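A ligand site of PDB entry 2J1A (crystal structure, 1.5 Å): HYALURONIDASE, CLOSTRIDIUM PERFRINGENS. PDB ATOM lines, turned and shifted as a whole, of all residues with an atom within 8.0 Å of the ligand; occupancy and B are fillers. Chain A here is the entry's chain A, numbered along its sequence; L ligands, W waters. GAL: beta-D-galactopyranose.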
ATOM      1  N   GLU A  20      15.006  19.736 -16.096  1.00  0.00           N
ATOM      2  CA  GLU A  20      13.960  20.742 -16.227  1.00  0.00           C
ATOM      3  C   GLU A  20      14.094  21.403 -17.603  1.00  0.00           C
ATOM      4  O   GLU A  20      15.157  21.950 -17.889  1.00  0.00           O
ATOM      5  CB  GLU A  20      14.111  21.825 -15.140  1.00  0.00           C
ATOM      6  CG  GLU A  20      12.991  22.844 -15.238  1.00  0.00           C
ATOM      7  CD  GLU A  20      11.596  22.211 -15.012  1.00  0.00           C
ATOM      8  OE1 GLU A  20      11.427  21.399 -14.062  1.00  0.00           O
ATOM      9  OE2 GLU A  20      10.683  22.530 -15.836  1.00  0.00           O
ATOM     10  N   GLY A  23       9.802  24.870 -16.994  1.00  0.00           N
ATOM     11  CA  GLY A  23       9.848  26.085 -16.156  1.00  0.00           C
ATOM     12  C   GLY A  23      11.064  26.996 -16.421  1.00  0.00           C
ATOM     13  O   GLY A  23      11.017  28.211 -16.186  1.00  0.00           O
ATOM     14  N   GLU A  24      12.134  26.395 -16.936  1.00  0.00           N
ATOM     15  CA  GLU A  24      13.335  27.084 -17.384  1.00  0.00           C
ATOM     16  C   GLU A  24      14.087  26.064 -18.237  1.00  0.00           C
ATOM     17  O   GLU A  24      13.716  24.893 -18.256  1.00  0.00           O
ATOM     18  CB  GLU A  24      14.218  27.559 -16.204  1.00  0.00           C
ATOM     19  CG  GLU A  24      14.805  26.452 -15.307  1.00  0.00           C
ATOM     20  CD  GLU A  24      15.432  27.001 -14.013  1.00  0.00           C
ATOM     21  OE1 GLU A  24      16.030  28.126 -14.063  1.00  0.00           O
ATOM     22  OE2 GLU A  24      15.257  26.349 -12.946  1.00  0.00           O
ATOM     23  N   ALA A  26      17.004  23.955 -18.280  1.00  0.00           N
ATOM     24  CA  ALA A  26      18.087  23.440 -17.429  1.00  0.00           C
ATOM     25  C   ALA A  26      18.385  21.945 -17.678  1.00  0.00           C
ATOM     26  O   ALA A  26      18.351  21.144 -16.732  1.00  0.00           O
ATOM     27  CB  ALA A  26      17.764  23.684 -15.947  1.00  0.00           C
ATOM     28  N   PHE A  39      23.183  25.745 -15.792  1.00  0.00           N
ATOM     29  CA  PHE A  39      23.143  24.641 -14.846  1.00  0.00           C
ATOM     30  C   PHE A  39      22.089  23.626 -15.277  1.00  0.00           C
ATOM     31  O   PHE A  39      21.090  23.966 -15.965  1.00  0.00           O
ATOM     32  CB  PHE A  39      22.889  25.144 -13.435  1.00  0.00           C
ATOM     33  CG  PHE A  39      21.645  25.971 -13.302  1.00  0.00           C
ATOM     34  CD1 PHE A  39      20.406  25.346 -13.073  1.00  0.00           C
ATOM     35  CD2 PHE A  39      21.696  27.376 -13.386  1.00  0.00           C
ATOM     36  CE1 PHE A  39      19.241  26.091 -12.941  1.00  0.00           C
ATOM     37  CE2 PHE A  39      20.521  28.132 -13.263  1.00  0.00           C
ATOM     38  CZ  PHE A  39      19.297  27.474 -13.036  1.00  0.00           C
ATOM     39  N   TRP A  40      22.363  22.371 -14.931  1.00  0.00           N
ATOM     40  CA  TRP A  40      21.370  21.310 -14.965  1.00  0.00           C
ATOM     41  C   TRP A  40      20.510  21.518 -13.712  1.00  0.00           C
ATOM     42  O   TRP A  40      21.025  21.849 -12.625  1.00  0.00           O
ATOM     43  CB  TRP A  40      22.060  19.937 -14.902  1.00  0.00           C
ATOM     44  CG  TRP A  40      21.139  18.825 -14.409  1.00  0.00           C
ATOM     45  CD1 TRP A  40      20.022  18.354 -15.050  1.00  0.00           C
ATOM     46  CD2 TRP A  40      21.275  18.044 -13.209  1.00  0.00           C
ATOM     47  NE1 TRP A  40      19.442  17.327 -14.325  1.00  0.00           N
ATOM     48  CE2 TRP A  40      20.200  17.109 -13.183  1.00  0.00           C
ATOM     49  CE3 TRP A  40      22.205  18.039 -12.155  1.00  0.00           C
ATOM     50  CZ2 TRP A  40      20.018  16.183 -12.146  1.00  0.00           C
ATOM     51  CZ3 TRP A  40      22.008  17.107 -11.084  1.00  0.00           C
ATOM     52  CH2 TRP A  40      20.917  16.193 -11.106  1.00  0.00           C
ATOM     53  N   HIS A  41      19.199  21.287 -13.839  1.00  0.00           N
ATOM     54  CA  HIS A  41      18.326  21.230 -12.656  1.00  0.00           C
ATOM     55  C   HIS A  41      17.472  19.978 -12.842  1.00  0.00           C
ATOM     56  O   HIS A  41      16.983  19.712 -13.956  1.00  0.00           O
ATOM     57  CB  HIS A  41      17.373  22.474 -12.639  1.00  0.00           C
ATOM     58  CG  HIS A  41      16.793  22.788 -11.286  1.00  0.00           C
ATOM     59  ND1 HIS A  41      16.144  21.855 -10.512  1.00  0.00           N
ATOM     60  CD2 HIS A  41      16.746  23.949 -10.583  1.00  0.00           C
ATOM     61  CE1 HIS A  41      15.769  22.401  -9.366  1.00  0.00           C
ATOM     62  NE2 HIS A  41      16.087  23.688  -9.402  1.00  0.00           N
ATOM     63  N   SER A  42      17.375  19.172 -11.783  1.00  0.00           N
ATOM     64  CA  SER A  42      16.329  18.137 -11.667  1.00  0.00           C
ATOM     65  C   SER A  42      14.969  18.771 -12.035  1.00  0.00           C
ATOM     66  O   SER A  42      14.760  19.986 -11.844  1.00  0.00           O
ATOM     67  CB  SER A  42      16.251  17.615 -10.214  1.00  0.00           C
ATOM     68  OG  SER A  42      16.032  18.691  -9.305  1.00  0.00           O
ATOM     69  N   LYS A  43      14.029  17.968 -12.535  1.00  0.00           N
ATOM     70  CA  LYS A  43      12.718  18.543 -12.920  1.00  0.00           C
ATOM     71  C   LYS A  43      12.001  19.023 -11.671  1.00  0.00           C
ATOM     72  O   LYS A  43      11.702  18.208 -10.759  1.00  0.00           O
ATOM     73  CB  LYS A  43      11.866  17.512 -13.652  1.00  0.00           C
ATOM     74  CG  LYS A  43      10.516  18.028 -14.089  1.00  0.00           C
ATOM     75  CD  LYS A  43       9.823  17.002 -15.042  1.00  0.00           C
ATOM     76  CE  LYS A  43       8.362  17.403 -15.304  1.00  0.00           C
ATOM     77  NZ  LYS A  43       8.176  18.828 -15.651  1.00  0.00           N
ATOM     78  N   TRP A  44      11.741  20.329 -11.625  1.00  0.00           N
ATOM     79  CA  TRP A  44      10.988  20.938 -10.526  1.00  0.00           C
ATOM     80  C   TRP A  44       9.572  21.385 -10.930  1.00  0.00           C
ATOM     81  O   TRP A  44       8.710  21.480 -10.059  1.00  0.00           O
ATOM     82  CB  TRP A  44      11.784  22.113  -9.891  1.00  0.00           C
ATOM     83  CG  TRP A  44      12.088  23.269 -10.845  1.00  0.00           C
ATOM     84  CD1 TRP A  44      13.287  23.531 -11.512  1.00  0.00           C
ATOM     85  CD2 TRP A  44      11.197  24.340 -11.209  1.00  0.00           C
ATOM     86  NE1 TRP A  44      13.163  24.690 -12.269  1.00  0.00           N
ATOM     87  CE2 TRP A  44      11.891  25.188 -12.121  1.00  0.00           C
ATOM     88  CE3 TRP A  44       9.852  24.637 -10.879  1.00  0.00           C
ATOM     89  CZ2 TRP A  44      11.294  26.336 -12.691  1.00  0.00           C
ATOM     90  CZ3 TRP A  44       9.246  25.786 -11.448  1.00  0.00           C
ATOM     91  CH2 TRP A  44       9.972  26.621 -12.344  1.00  0.00           C
ATOM     92  N   SER A  45       9.345  21.627 -12.228  1.00  0.00           N
ATOM     93  CA  SER A  45       7.992  21.960 -12.700  1.00  0.00           C
ATOM     94  C   SER A  45       7.054  20.761 -12.527  1.00  0.00           C
ATOM     95  O   SER A  45       7.460  19.611 -12.644  1.00  0.00           O
ATOM     96  CB  SER A  45       7.960  22.447 -14.163  1.00  0.00           C
ATOM     97  OG  SER A  45       8.393  21.453 -15.041  1.00  0.00           O
ATOM     98  N   ARG A  73      25.515  25.549  -8.863  1.00  0.00           N
ATOM     99  CA  ARG A  73      24.924  26.733  -9.497  1.00  0.00           C
ATOM    100  C   ARG A  73      25.272  27.965  -8.652  1.00  0.00           C
ATOM    101  O   ARG A  73      25.368  27.890  -7.427  1.00  0.00           O
ATOM    102  CB  ARG A  73      23.411  26.624  -9.774  1.00  0.00           C
ATOM    103  CG  ARG A  73      22.557  26.865  -8.635  1.00  0.00           C
ATOM    104  CD  ARG A  73      21.068  26.626  -9.014  1.00  0.00           C
ATOM    105  NE  ARG A  73      20.378  27.790  -9.549  1.00  0.00           N
ATOM    106  CZ  ARG A  73      19.035  27.826  -9.688  1.00  0.00           C
ATOM    107  NH1 ARG A  73      18.313  26.735  -9.374  1.00  0.00           N
ATOM    108  NH2 ARG A  73      18.418  28.890 -10.182  1.00  0.00           N
ATOM    109  N   ASP A  75      23.789  31.126  -8.683  1.00  0.00           N
ATOM    110  CA  ASP A  75      22.730  32.137  -8.416  1.00  0.00           C
ATOM    111  C   ASP A  75      21.744  31.758  -7.295  1.00  0.00           C
ATOM    112  O   ASP A  75      20.904  32.592  -6.908  1.00  0.00           O
ATOM    113  CB  ASP A  75      21.955  32.399  -9.699  1.00  0.00           C
ATOM    114  CG  ASP A  75      21.131  31.200 -10.115  1.00  0.00           C
ATOM    115  OD1 ASP A  75      21.721  30.108 -10.347  1.00  0.00           O
ATOM    116  OD2 ASP A  75      19.877  31.319 -10.171  1.00  0.00           O
ATOM    117  N   SER A  76      21.783  30.504  -6.825  1.00  0.00           N
ATOM    118  CA  SER A  76      20.808  30.005  -5.834  1.00  0.00           C
ATOM    119  C   SER A  76      21.367  28.768  -5.162  1.00  0.00           C
ATOM    120  O   SER A  76      22.186  28.055  -5.782  1.00  0.00           O
ATOM    121  CB  SER A  76      19.482  29.643  -6.533  1.00  0.00           C
ATOM    122  OG  SER A  76      18.638  28.820  -5.738  1.00  0.00           O
ATOM    123  N   LYS A  77      20.923  28.467  -3.946  1.00  0.00           N
ATOM    124  CA  LYS A  77      21.360  27.224  -3.324  1.00  0.00           C
ATOM    125  C   LYS A  77      20.437  26.014  -3.651  1.00  0.00           C
ATOM    126  O   LYS A  77      20.694  24.920  -3.194  1.00  0.00           O
ATOM    127  CB  LYS A  77      21.584  27.390  -1.814  1.00  0.00           C
ATOM    128  CG  LYS A  77      20.388  27.350  -0.972  1.00  0.00           C
ATOM    129  CD  LYS A  77      20.646  27.942   0.468  1.00  0.00           C
ATOM    130  CE  LYS A  77      22.035  27.567   1.006  1.00  0.00           C
ATOM    131  NZ  LYS A  77      22.104  27.246   2.477  1.00  0.00           N
ATOM    132  N   ASN A  78      19.369  26.258  -4.414  1.00  0.00           N
ATOM    133  CA  ASN A  78      18.401  25.208  -4.728  1.00  0.00           C
ATOM    134  C   ASN A  78      19.109  24.081  -5.438  1.00  0.00           C
ATOM    135  O   ASN A  78      19.677  24.282  -6.499  1.00  0.00           O
ATOM    136  CB  ASN A  78      17.314  25.737  -5.680  1.00  0.00           C
ATOM    137  CG  ASN A  78      16.231  26.535  -4.945  1.00  0.00           C
ATOM    138  OD1 ASN A  78      15.308  27.090  -5.561  1.00  0.00           O
ATOM    139  ND2 ASN A  78      16.355  26.603  -3.628  1.00  0.00           N
ATOM    140  N   GLY A  79      19.090  22.904  -4.838  1.00  0.00           N
ATOM    141  CA  GLY A  79      19.707  21.717  -5.428  1.00  0.00           C
ATOM    142  C   GLY A  79      21.201  21.553  -5.189  1.00  0.00           C
ATOM    143  O   GLY A  79      21.806  20.604  -5.703  1.00  0.00           O
ATOM    144  N   SER A 131      18.370  23.874  -0.179  1.00  0.00           N
ATOM    145  CA  SER A 131      17.560  24.776  -0.989  1.00  0.00           C
ATOM    146  C   SER A 131      17.470  26.116  -0.284  1.00  0.00           C
ATOM    147  O   SER A 131      17.770  26.201   0.910  1.00  0.00           O
ATOM    148  CB  SER A 131      16.156  24.189  -1.220  1.00  0.00           C
ATOM    149  OG  SER A 131      15.529  23.988   0.035  1.00  0.00           O
ATOM    150  N   ASP A 132      17.048  27.159  -0.994  1.00  0.00           N
ATOM    151  CA  ASP A 132      16.850  28.467  -0.411  1.00  0.00           C
ATOM    152  C   ASP A 132      15.779  28.433   0.673  1.00  0.00           C
ATOM    153  O   ASP A 132      15.867  29.145   1.672  1.00  0.00           O
ATOM    154  CB  ASP A 132      16.467  29.494  -1.483  1.00  0.00           C
ATOM    155  CG  ASP A 132      17.539  29.640  -2.542  1.00  0.00           C
ATOM    156  OD1 ASP A 132      18.735  29.556  -2.202  1.00  0.00           O
ATOM    157  OD2 ASP A 132      17.284  29.852  -3.743  1.00  0.00           O
ATOM    158  N   GLN A 133      14.762  27.598   0.473  1.00  0.00           N
ATOM    159  CA  GLN A 133      13.563  27.619   1.304  1.00  0.00           C
ATOM    160  C   GLN A 133      13.811  26.941   2.644  1.00  0.00           C
ATOM    161  O   GLN A 133      14.425  25.873   2.711  1.00  0.00           O
ATOM    162  CB  GLN A 133      12.399  26.948   0.577  1.00  0.00           C
ATOM    163  CG  GLN A 133      12.804  25.765  -0.291  1.00  0.00           C
ATOM    164  CD  GLN A 133      11.605  25.046  -0.879  1.00  0.00           C
ATOM    165  OE1 GLN A 133      10.944  24.271  -0.199  1.00  0.00           O
ATOM    166  NE2 GLN A 133      11.341  25.295  -2.161  1.00  0.00           N
ATOM    167  N   PHE A 140      15.581  18.922  -4.671  1.00  0.00           N
ATOM    168  CA  PHE A 140      16.173  19.351  -5.917  1.00  0.00           C
ATOM    169  C   PHE A 140      17.620  18.899  -6.047  1.00  0.00           C
ATOM    170  O   PHE A 140      18.314  18.623  -5.043  1.00  0.00           O
ATOM    171  CB  PHE A 140      16.232  20.889  -5.956  1.00  0.00           C
ATOM    172  CG  PHE A 140      14.928  21.571  -5.685  1.00  0.00           C
ATOM    173  CD1 PHE A 140      14.853  22.570  -4.698  1.00  0.00           C
ATOM    174  CD2 PHE A 140      13.784  21.221  -6.407  1.00  0.00           C
ATOM    175  CE1 PHE A 140      13.623  23.220  -4.440  1.00  0.00           C
ATOM    176  CE2 PHE A 140      12.557  21.850  -6.169  1.00  0.00           C
ATOM    177  CZ  PHE A 140      12.474  22.870  -5.191  1.00  0.00           C
ATOM    178  N   ALA A 141      18.106  18.908  -7.291  1.00  0.00           N
ATOM    179  CA  ALA A 141      19.556  18.784  -7.523  1.00  0.00           C
ATOM    180  C   ALA A 141      19.938  19.642  -8.705  1.00  0.00           C
ATOM    181  O   ALA A 141      19.240  19.687  -9.701  1.00  0.00           O
ATOM    182  CB  ALA A 141      19.978  17.362  -7.777  1.00  0.00           C
ATOM    183  N   THR A 142      21.008  20.409  -8.492  1.00  0.00           N
ATOM    184  CA  THR A 142      21.557  21.228  -9.570  1.00  0.00           C
ATOM    185  C   THR A 142      23.087  21.141  -9.665  1.00  0.00           C
ATOM    186  O   THR A 142      23.795  20.822  -8.663  1.00  0.00           O
ATOM    187  CB  THR A 142      21.167  22.724  -9.376  1.00  0.00           C
ATOM    188  OG1 THR A 142      21.600  23.131  -8.063  1.00  0.00           O
ATOM    189  CG2 THR A 142      19.622  22.893  -9.494  1.00  0.00           C
HETATM  190  C1  GAL L   1      13.378  28.971  -8.398  1.00  0.00           C
HETATM  191  C2  GAL L   1      14.722  28.962  -9.174  1.00  0.00           C
HETATM  192  C3  GAL L   1      14.678  27.722 -10.093  1.00  0.00           C
HETATM  193  C4  GAL L   1      14.327  26.419  -9.339  1.00  0.00           C
HETATM  194  C5  GAL L   1      13.026  26.605  -8.536  1.00  0.00           C
HETATM  195  C6  GAL L   1      12.596  25.347  -7.749  1.00  0.00           C
HETATM  196  O1  GAL L   1      13.307  30.082  -7.557  1.00  0.00           O
HETATM  197  O2  GAL L   1      14.851  30.101  -9.995  1.00  0.00           O
HETATM  198  O3  GAL L   1      15.947  27.630 -10.751  1.00  0.00           O
HETATM  199  O4  GAL L   1      15.378  26.095  -8.428  1.00  0.00           O
HETATM  200  O5  GAL L   1      13.174  27.726  -7.683  1.00  0.00           O
HETATM  201  O6  GAL L   1      11.422  25.622  -7.002  1.00  0.00           O
HETATM  202  O   HOH W   1      11.347  26.696  -4.533  1.00  0.00           O
HETATM  203  O   HOH W   2      16.078  30.283 -12.341  1.00  0.00           O
HETATM  204  O   HOH W   3      14.701  30.108  -5.326  1.00  0.00           O
HETATM  205  O   HOH W   4       9.102  24.212  -6.973  1.00  0.00           O
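OE2 of Glu 24 is in hydrogen-bond range of O3 of the ligand (2.6 Å). An oxygen (O4) of the ligand sits at hydrogen-bond distance from a ring nitrogen (NE2) of His 41 (2.7 Å). An oxygen (O3) of the ligand sits at hydrogen-bond distance from the guanidinium group (NH2) of Arg 73 (2.8 Å). O4 of the ligand sits at hydrogen-bond distance from OD1 of Asn 78.
NE1 of Trp 44 lies within hydrogen-bond range of OE2 of Glu 24 (2.8 Å). O of Ala 26 is in hydrogen-bond range of N of His 41 (3.0 Å). OG of Ser 42 is in hydrogen-bond range of ND1 of His 41 (3.4 Å). O of His 41 sits at hydrogen-bond distance from N of Glu 20. The side-chain carboxylate (OD1) of Asp 75 is in salt-bridge range of the guanidinium group (NE) of Arg 73 (2.8 Å). The backbone NH of Asn 78 sits at hydrogen-bond distance from the side-chain hydroxyl of Ser 76 (3.0 Å). The backbone carbonyl oxygen (O) of Asn 78 sits at hydrogen-bond distance from the side-chain hydroxyl (OG1) of Thr 142, at 2.7 Å. N of Trp 44 sits at hydrogen-bond distance from OE1 of Glu 20.
NE1 of Trp 44 touches C4 of the ligand, at 3.6 Å. Phe 140 touches the ligand. Hydrophobic or aromatic side chains that line the ligand: His 41, Trp 44 and Phe 140. Of the 23 residues printed, 6 come within 4 Å of the ligand. Along chain A the residues within 4 Å of the ligand span positions 24 to 140. The nearest printed residue that does not touch the ligand is Phe 39 (4.1 Å).
Water W3 lies within hydrogen-bond range of an oxygen (O1) of the ligand (2.6 Å), the side-chain carboxylate of Asp 132 (3.0 Å) and the side-chain amide oxygen of Asn 78 (3.1 Å). Water W2 lies within hydrogen-bond range of O2 of the ligand (2.7 Å), OE1 of Glu 24 (2.8 Å) and NH2 of Arg 73 (3.5 Å). Water W1 bridges an oxygen (O6) of the ligand (2.7 Å) and the side-chain amide nitrogen of Gln 133 (2.8 Å).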
